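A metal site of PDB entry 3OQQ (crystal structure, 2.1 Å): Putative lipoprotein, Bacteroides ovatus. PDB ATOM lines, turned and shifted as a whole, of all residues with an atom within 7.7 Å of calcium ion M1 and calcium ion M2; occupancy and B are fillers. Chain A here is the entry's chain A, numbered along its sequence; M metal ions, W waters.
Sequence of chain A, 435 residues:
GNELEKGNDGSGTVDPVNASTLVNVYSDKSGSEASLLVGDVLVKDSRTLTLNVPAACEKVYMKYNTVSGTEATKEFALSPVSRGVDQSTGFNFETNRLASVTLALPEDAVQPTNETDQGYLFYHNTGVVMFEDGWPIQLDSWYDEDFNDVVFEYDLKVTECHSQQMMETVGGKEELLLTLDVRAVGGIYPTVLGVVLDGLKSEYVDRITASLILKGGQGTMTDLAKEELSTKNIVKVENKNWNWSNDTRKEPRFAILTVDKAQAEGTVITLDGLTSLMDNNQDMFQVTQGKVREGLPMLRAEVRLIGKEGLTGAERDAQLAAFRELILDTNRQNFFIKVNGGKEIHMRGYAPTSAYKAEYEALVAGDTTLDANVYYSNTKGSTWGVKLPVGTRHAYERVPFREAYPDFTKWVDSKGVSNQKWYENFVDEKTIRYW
O of Val 287 lies within hydrogen-bond range of N of Glu 397. The backbone NH (N) of Asp 133 lies close to the side-chain carboxylate (OD2) of Asp 149. The backbone carbonyl oxygen of Ala 395 is in hydrogen-bond range of the side-chain amide nitrogen of Asn 148 (2.8 Å). N of Asp 149 lies within hydrogen-bond range of O of Phe 131. The side-chain carboxylate of Glu 132 sits close to the backbone NH of Phe 147 (2.9 Å). The side-chain carboxylate (OD2) of Asp 146 sits close to the backbone NH (N) of Arg 398 (2.8 Å).
Within 4 Å of calcium ion M1: Asp 146, Asn 148, Asp 149, Gly 186 and Glu 397.
Within 4 Å of calcium ion M2: Glu 132, Asp 146 and Asp 149. Along chain A the residues within 4 Å of calcium ion M2 span positions 132 to 149. The nearest printed residue that does not touch calcium ion M2 is Phe 147 (4.4 Å).
The backbone carbonyl oxygen (O) of Gly 186 is bound to calcium ion M1, at 2.4 Å. OD1 of Asn 148 binds calcium ion M1 (2.4 Å). Calcium ion M1 is bound by OE1 of Glu 397 (2.4 Å). The side-chain carboxylate (OD2) of Asp 146 binds calcium ion M1 (2.4 Å). The side-chain carboxylate (OD1) of Asp 149 binds calcium ion M1 (2.5 Å). OE2 of Glu 397 is bound to calcium ion M1. Calcium ion M1 is bound by water W3, at 2.7 Å. Calcium ion M1 is bound by OD1 of Asp 146 (2.7 Å). Calcium ion M1 has eight donor atoms within binding distance.
Calcium ion M2 is bound by OE2 of Glu 132 (2.2 Å), water W3 (2.4 Å), water W1 (2.4 Å), water W2 (2.4 Å), OE1 of Glu 132 (2.5 Å), OD2 of Asp 149 (2.5 Å), OD1 of Asp 146 (2.5 Å) and OD1 of Asp 149 (2.6 Å).
Water W2 bridges the side-chain carboxylate of Glu 145 and the backbone NH of Asp 146.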
ATOM      1  N   PHE A 131     -25.204 -12.349  21.520  1.00  0.00           N
ATOM      2  CA  PHE A 131     -24.544 -11.050  21.424  1.00  0.00           C
ATOM      3  C   PHE A 131     -23.116 -11.133  20.992  1.00  0.00           C
ATOM      4  O   PHE A 131     -22.430 -12.100  21.305  1.00  0.00           O
ATOM      5  CB  PHE A 131     -24.562 -10.366  22.805  1.00  0.00           C
ATOM      6  CG  PHE A 131     -25.710  -9.433  23.001  1.00  0.00           C
ATOM      7  CD1 PHE A 131     -25.722  -8.176  22.408  1.00  0.00           C
ATOM      8  CD2 PHE A 131     -26.779  -9.802  23.810  1.00  0.00           C
ATOM      9  CE1 PHE A 131     -26.792  -7.304  22.611  1.00  0.00           C
ATOM     10  CE2 PHE A 131     -27.871  -8.939  23.988  1.00  0.00           C
ATOM     11  CZ  PHE A 131     -27.861  -7.693  23.395  1.00  0.00           C
ATOM     12  N   GLU A 132     -22.659 -10.059  20.325  1.00  0.00           N
ATOM     13  CA  GLU A 132     -21.280  -9.713  19.981  1.00  0.00           C
ATOM     14  C   GLU A 132     -20.843  -8.718  21.053  1.00  0.00           C
ATOM     15  O   GLU A 132     -21.640  -7.886  21.466  1.00  0.00           O
ATOM     16  CB  GLU A 132     -21.180  -9.140  18.551  1.00  0.00           C
ATOM     17  CG  GLU A 132     -20.815 -10.197  17.515  1.00  0.00           C
ATOM     18  CD  GLU A 132     -19.503 -10.905  17.813  1.00  0.00           C
ATOM     19  OE1 GLU A 132     -18.466 -10.216  17.823  1.00  0.00           O
ATOM     20  OE2 GLU A 132     -19.514 -12.139  18.054  1.00  0.00           O
ATOM     21  N   ASP A 133     -19.602  -8.805  21.528  1.00  0.00           N
ATOM     22  CA  ASP A 133     -19.123  -7.967  22.625  1.00  0.00           C
ATOM     23  C   ASP A 133     -18.244  -6.795  22.203  1.00  0.00           C
ATOM     24  O   ASP A 133     -17.715  -6.103  23.066  1.00  0.00           O
ATOM     25  CB  ASP A 133     -18.327  -8.844  23.621  1.00  0.00           C
ATOM     26  CG  ASP A 133     -17.134  -9.590  23.042  1.00  0.00           C
ATOM     27  OD1 ASP A 133     -16.607  -9.185  21.976  1.00  0.00           O
ATOM     28  OD2 ASP A 133     -16.753 -10.631  23.618  1.00  0.00           O
ATOM     29  N   GLY A 134     -18.042  -6.607  20.917  1.00  0.00           N
ATOM     30  CA  GLY A 134     -17.091  -5.622  20.400  1.00  0.00           C
ATOM     31  C   GLY A 134     -17.557  -4.217  20.142  1.00  0.00           C
ATOM     32  O   GLY A 134     -16.705  -3.370  19.855  1.00  0.00           O
ATOM     33  N   ASP A 144     -19.774 -12.067   9.802  1.00  0.00           N
ATOM     34  CA  ASP A 144     -18.548 -12.851   9.804  1.00  0.00           C
ATOM     35  C   ASP A 144     -18.065 -12.989  11.278  1.00  0.00           C
ATOM     36  O   ASP A 144     -17.143 -13.737  11.577  1.00  0.00           O
ATOM     37  CB  ASP A 144     -17.470 -12.214   8.911  1.00  0.00           C
ATOM     38  CG  ASP A 144     -17.440 -12.780   7.494  1.00  0.00           C
ATOM     39  OD1 ASP A 144     -17.952 -13.904   7.290  1.00  0.00           O
ATOM     40  OD2 ASP A 144     -16.857 -12.136   6.616  1.00  0.00           O
ATOM     41  N   GLU A 145     -18.722 -12.239  12.200  1.00  0.00           N
ATOM     42  CA  GLU A 145     -18.517 -12.362  13.652  1.00  0.00           C
ATOM     43  C   GLU A 145     -19.126 -13.678  14.075  1.00  0.00           C
ATOM     44  O   GLU A 145     -19.964 -14.199  13.331  1.00  0.00           O
ATOM     45  CB  GLU A 145     -19.160 -11.174  14.428  1.00  0.00           C
ATOM     46  CG  GLU A 145     -18.642  -9.781  14.082  1.00  0.00           C
ATOM     47  CD  GLU A 145     -17.205  -9.418  14.422  1.00  0.00           C
ATOM     48  OE1 GLU A 145     -16.419 -10.314  14.796  1.00  0.00           O
ATOM     49  OE2 GLU A 145     -16.863  -8.227  14.270  1.00  0.00           O
ATOM     50  N   ASP A 146     -18.720 -14.252  15.241  1.00  0.00           N
ATOM     51  CA  ASP A 146     -19.242 -15.552  15.645  1.00  0.00           C
ATOM     52  C   ASP A 146     -20.595 -15.500  16.427  1.00  0.00           C
ATOM     53  O   ASP A 146     -21.267 -16.533  16.514  1.00  0.00           O
ATOM     54  CB  ASP A 146     -18.173 -16.378  16.430  1.00  0.00           C
ATOM     55  CG  ASP A 146     -17.526 -15.797  17.679  1.00  0.00           C
ATOM     56  OD1 ASP A 146     -17.954 -14.701  18.129  1.00  0.00           O
ATOM     57  OD2 ASP A 146     -16.601 -16.421  18.212  1.00  0.00           O
ATOM     58  N   PHE A 147     -20.973 -14.330  16.950  1.00  0.00           N
ATOM     59  CA  PHE A 147     -22.228 -14.102  17.704  1.00  0.00           C
ATOM     60  C   PHE A 147     -22.423 -15.098  18.861  1.00  0.00           C
ATOM     61  O   PHE A 147     -23.550 -15.514  19.125  1.00  0.00           O
ATOM     62  CB  PHE A 147     -23.472 -14.106  16.776  1.00  0.00           C
ATOM     63  CG  PHE A 147     -23.693 -12.748  16.142  1.00  0.00           C
ATOM     64  CD1 PHE A 147     -23.010 -12.396  14.965  1.00  0.00           C
ATOM     65  CD2 PHE A 147     -24.521 -11.808  16.737  1.00  0.00           C
ATOM     66  CE1 PHE A 147     -23.183 -11.126  14.397  1.00  0.00           C
ATOM     67  CE2 PHE A 147     -24.694 -10.538  16.170  1.00  0.00           C
ATOM     68  CZ  PHE A 147     -24.018 -10.198  15.011  1.00  0.00           C
ATOM     69  N   ASN A 148     -21.348 -15.444  19.564  1.00  0.00           N
ATOM     70  CA  ASN A 148     -21.503 -16.358  20.705  1.00  0.00           C
ATOM     71  C   ASN A 148     -20.866 -15.761  21.967  1.00  0.00           C
ATOM     72  O   ASN A 148     -20.670 -16.471  22.943  1.00  0.00           O
ATOM     73  CB  ASN A 148     -20.917 -17.732  20.385  1.00  0.00           C
ATOM     74  CG  ASN A 148     -19.413 -17.648  20.236  1.00  0.00           C
ATOM     75  OD1 ASN A 148     -18.826 -16.598  20.487  1.00  0.00           O
ATOM     76  ND2 ASN A 148     -18.773 -18.741  19.868  1.00  0.00           N
ATOM     77  N   ASP A 149     -20.485 -14.463  21.911  1.00  0.00           N
ATOM     78  CA  ASP A 149     -19.798 -13.771  23.007  1.00  0.00           C
ATOM     79  C   ASP A 149     -20.569 -13.846  24.304  1.00  0.00           C
ATOM     80  O   ASP A 149     -19.959 -14.012  25.365  1.00  0.00           O
ATOM     81  CB  ASP A 149     -19.452 -12.340  22.611  1.00  0.00           C
ATOM     82  CG  ASP A 149     -18.597 -12.341  21.346  1.00  0.00           C
ATOM     83  OD1 ASP A 149     -18.122 -13.450  20.938  1.00  0.00           O
ATOM     84  OD2 ASP A 149     -18.415 -11.276  20.749  1.00  0.00           O
ATOM     85  N   VAL A 150     -21.916 -13.771  24.213  1.00  0.00           N
ATOM     86  CA  VAL A 150     -22.844 -14.016  25.301  1.00  0.00           C
ATOM     87  C   VAL A 150     -24.034 -14.724  24.661  1.00  0.00           C
ATOM     88  O   VAL A 150     -24.630 -14.228  23.699  1.00  0.00           O
ATOM     89  CB  VAL A 150     -23.298 -12.837  26.215  1.00  0.00           C
ATOM     90  CG1 VAL A 150     -24.146 -13.354  27.380  1.00  0.00           C
ATOM     91  CG2 VAL A 150     -22.100 -12.040  26.753  1.00  0.00           C
ATOM     92  N   VAL A 185     -20.383 -18.204  26.957  1.00  0.00           N
ATOM     93  CA  VAL A 185     -19.705 -16.914  27.006  1.00  0.00           C
ATOM     94  C   VAL A 185     -18.457 -17.050  26.108  1.00  0.00           C
ATOM     95  O   VAL A 185     -17.410 -17.507  26.555  1.00  0.00           O
ATOM     96  CB  VAL A 185     -19.386 -16.385  28.429  1.00  0.00           C
ATOM     97  CG1 VAL A 185     -18.794 -14.976  28.379  1.00  0.00           C
ATOM     98  CG2 VAL A 185     -20.628 -16.397  29.317  1.00  0.00           C
ATOM     99  N   GLY A 186     -18.606 -16.705  24.833  1.00  0.00           N
ATOM    100  CA  GLY A 186     -17.539 -16.786  23.837  1.00  0.00           C
ATOM    101  C   GLY A 186     -16.686 -15.539  23.778  1.00  0.00           C
ATOM    102  O   GLY A 186     -16.294 -15.102  22.710  1.00  0.00           O
ATOM    103  N   GLY A 187     -16.426 -14.946  24.930  1.00  0.00           N
ATOM    104  CA  GLY A 187     -15.619 -13.728  24.970  1.00  0.00           C
ATOM    105  C   GLY A 187     -14.854 -13.691  26.261  1.00  0.00           C
ATOM    106  O   GLY A 187     -15.298 -14.286  27.239  1.00  0.00           O
ATOM    107  N   ILE A 188     -13.724 -12.950  26.250  1.00  0.00           N
ATOM    108  CA  ILE A 188     -12.837 -12.794  27.400  1.00  0.00           C
ATOM    109  C   ILE A 188     -13.386 -11.724  28.348  1.00  0.00           C
ATOM    110  O   ILE A 188     -13.294 -11.892  29.566  1.00  0.00           O
ATOM    111  CB  ILE A 188     -11.398 -12.433  26.888  1.00  0.00           C
ATOM    112  CG1 ILE A 188     -10.759 -13.626  26.157  1.00  0.00           C
ATOM    113  CG2 ILE A 188     -10.472 -11.944  28.002  1.00  0.00           C
ATOM    114  CD1 ILE A 188      -9.893 -13.225  24.951  1.00  0.00           C
ATOM    115  N   MET A 284     -12.481 -20.203  26.958  1.00  0.00           N
ATOM    116  CA  MET A 284     -13.714 -19.476  27.268  1.00  0.00           C
ATOM    117  C   MET A 284     -14.813 -20.486  27.702  1.00  0.00           C
ATOM    118  O   MET A 284     -14.459 -21.554  28.206  1.00  0.00           O
ATOM    119  CB  MET A 284     -14.120 -18.534  26.119  1.00  0.00           C
ATOM    120  CG  MET A 284     -13.120 -17.355  25.954  1.00  0.00           C
ATOM    121  SD  MET A 284     -13.280 -16.488  24.232  1.00  0.00           S
ATOM    122  CE  MET A 284     -12.052 -17.520  23.323  1.00  0.00           C
ATOM    123  N   VAL A 287     -17.841 -22.844  24.120  1.00  0.00           N
ATOM    124  CA  VAL A 287     -17.665 -22.370  22.720  1.00  0.00           C
ATOM    125  C   VAL A 287     -16.488 -23.062  21.964  1.00  0.00           C
ATOM    126  O   VAL A 287     -16.365 -22.933  20.728  1.00  0.00           O
ATOM    127  CB  VAL A 287     -17.521 -20.804  22.639  1.00  0.00           C
ATOM    128  CG1 VAL A 287     -18.758 -20.092  23.156  1.00  0.00           C
ATOM    129  CG2 VAL A 287     -16.242 -20.284  23.335  1.00  0.00           C
ATOM    130  N   ALA A 395     -22.634 -20.772  17.452  1.00  0.00           N
ATOM    131  CA  ALA A 395     -21.432 -21.143  16.714  1.00  0.00           C
ATOM    132  C   ALA A 395     -20.257 -21.447  17.617  1.00  0.00           C
ATOM    133  O   ALA A 395     -20.115 -20.863  18.700  1.00  0.00           O
ATOM    134  CB  ALA A 395     -21.033 -20.002  15.789  1.00  0.00           C
ATOM    135  N   TYR A 396     -19.338 -22.291  17.100  1.00  0.00           N
ATOM    136  CA  TYR A 396     -18.045 -22.568  17.745  1.00  0.00           C
ATOM    137  C   TYR A 396     -17.238 -21.276  17.688  1.00  0.00           C
ATOM    138  O   TYR A 396     -17.487 -20.442  16.813  1.00  0.00           O
ATOM    139  CB  TYR A 396     -17.282 -23.694  17.010  1.00  0.00           C
ATOM    140  CG  TYR A 396     -17.726 -25.083  17.391  1.00  0.00           C
ATOM    141  CD1 TYR A 396     -17.405 -25.621  18.644  1.00  0.00           C
ATOM    142  CD2 TYR A 396     -18.397 -25.899  16.489  1.00  0.00           C
ATOM    143  CE1 TYR A 396     -17.823 -26.893  19.010  1.00  0.00           C
ATOM    144  CE2 TYR A 396     -18.795 -27.186  16.843  1.00  0.00           C
ATOM    145  CZ  TYR A 396     -18.518 -27.675  18.110  1.00  0.00           C
ATOM    146  OH  TYR A 396     -18.908 -28.939  18.465  1.00  0.00           O
ATOM    147  N   GLU A 397     -16.308 -21.080  18.629  1.00  0.00           N
ATOM    148  CA  GLU A 397     -15.487 -19.869  18.698  1.00  0.00           C
ATOM    149  C   GLU A 397     -14.785 -19.567  17.378  1.00  0.00           C
ATOM    150  O   GLU A 397     -14.196 -20.471  16.767  1.00  0.00           O
ATOM    151  CB  GLU A 397     -14.461 -19.960  19.835  1.00  0.00           C
ATOM    152  CG  GLU A 397     -13.879 -18.611  20.252  1.00  0.00           C
ATOM    153  CD  GLU A 397     -14.826 -17.458  20.561  1.00  0.00           C
ATOM    154  OE1 GLU A 397     -16.019 -17.707  20.858  1.00  0.00           O
ATOM    155  OE2 GLU A 397     -14.357 -16.298  20.521  1.00  0.00           O
ATOM    156  N   ARG A 398     -14.873 -18.285  16.946  1.00  0.00           N
ATOM    157  CA  ARG A 398     -14.282 -17.716  15.719  1.00  0.00           C
ATOM    158  C   ARG A 398     -14.864 -18.299  14.421  1.00  0.00           C
ATOM    159  O   ARG A 398     -14.353 -18.021  13.349  1.00  0.00           O
ATOM    160  CB  ARG A 398     -12.747 -17.835  15.723  1.00  0.00           C
ATOM    161  CG  ARG A 398     -12.057 -16.804  16.662  1.00  0.00           C
ATOM    162  CD  ARG A 398     -10.551 -17.034  16.745  1.00  0.00           C
ATOM    163  NE  ARG A 398     -10.229 -18.385  17.208  1.00  0.00           N
ATOM    164  CZ  ARG A 398     -10.118 -18.740  18.496  1.00  0.00           C
ATOM    165  NH1 ARG A 398     -10.252 -17.828  19.457  1.00  0.00           N
ATOM    166  NH2 ARG A 398      -9.855 -19.992  18.818  1.00  0.00           N
ATOM    167  N   VAL A 399     -15.962 -19.063  14.507  1.00  0.00           N
ATOM    168  CA  VAL A 399     -16.637 -19.538  13.294  1.00  0.00           C
ATOM    169  C   VAL A 399     -17.608 -18.418  12.855  1.00  0.00           C
ATOM    170  O   VAL A 399     -18.472 -18.032  13.647  1.00  0.00           O
ATOM    171  CB  VAL A 399     -17.369 -20.905  13.492  1.00  0.00           C
ATOM    172  CG1 VAL A 399     -18.295 -21.197  12.311  1.00  0.00           C
ATOM    173  CG2 VAL A 399     -16.382 -22.043  13.700  1.00  0.00           C
HETATM  174 CA    CA M   1     -16.737 -15.450  20.419  1.00  0.00          CA
HETATM  175 CA    CA M   2     -17.417 -12.295  18.671  1.00  0.00          CA
HETATM  176  O   HOH W   1     -15.906 -10.550  19.269  1.00  0.00           O
HETATM  177  O   HOH W   2     -16.507 -12.447  16.438  1.00  0.00           O
HETATM  178  O   HOH W   3     -15.457 -13.263  19.567  1.00  0.00           O
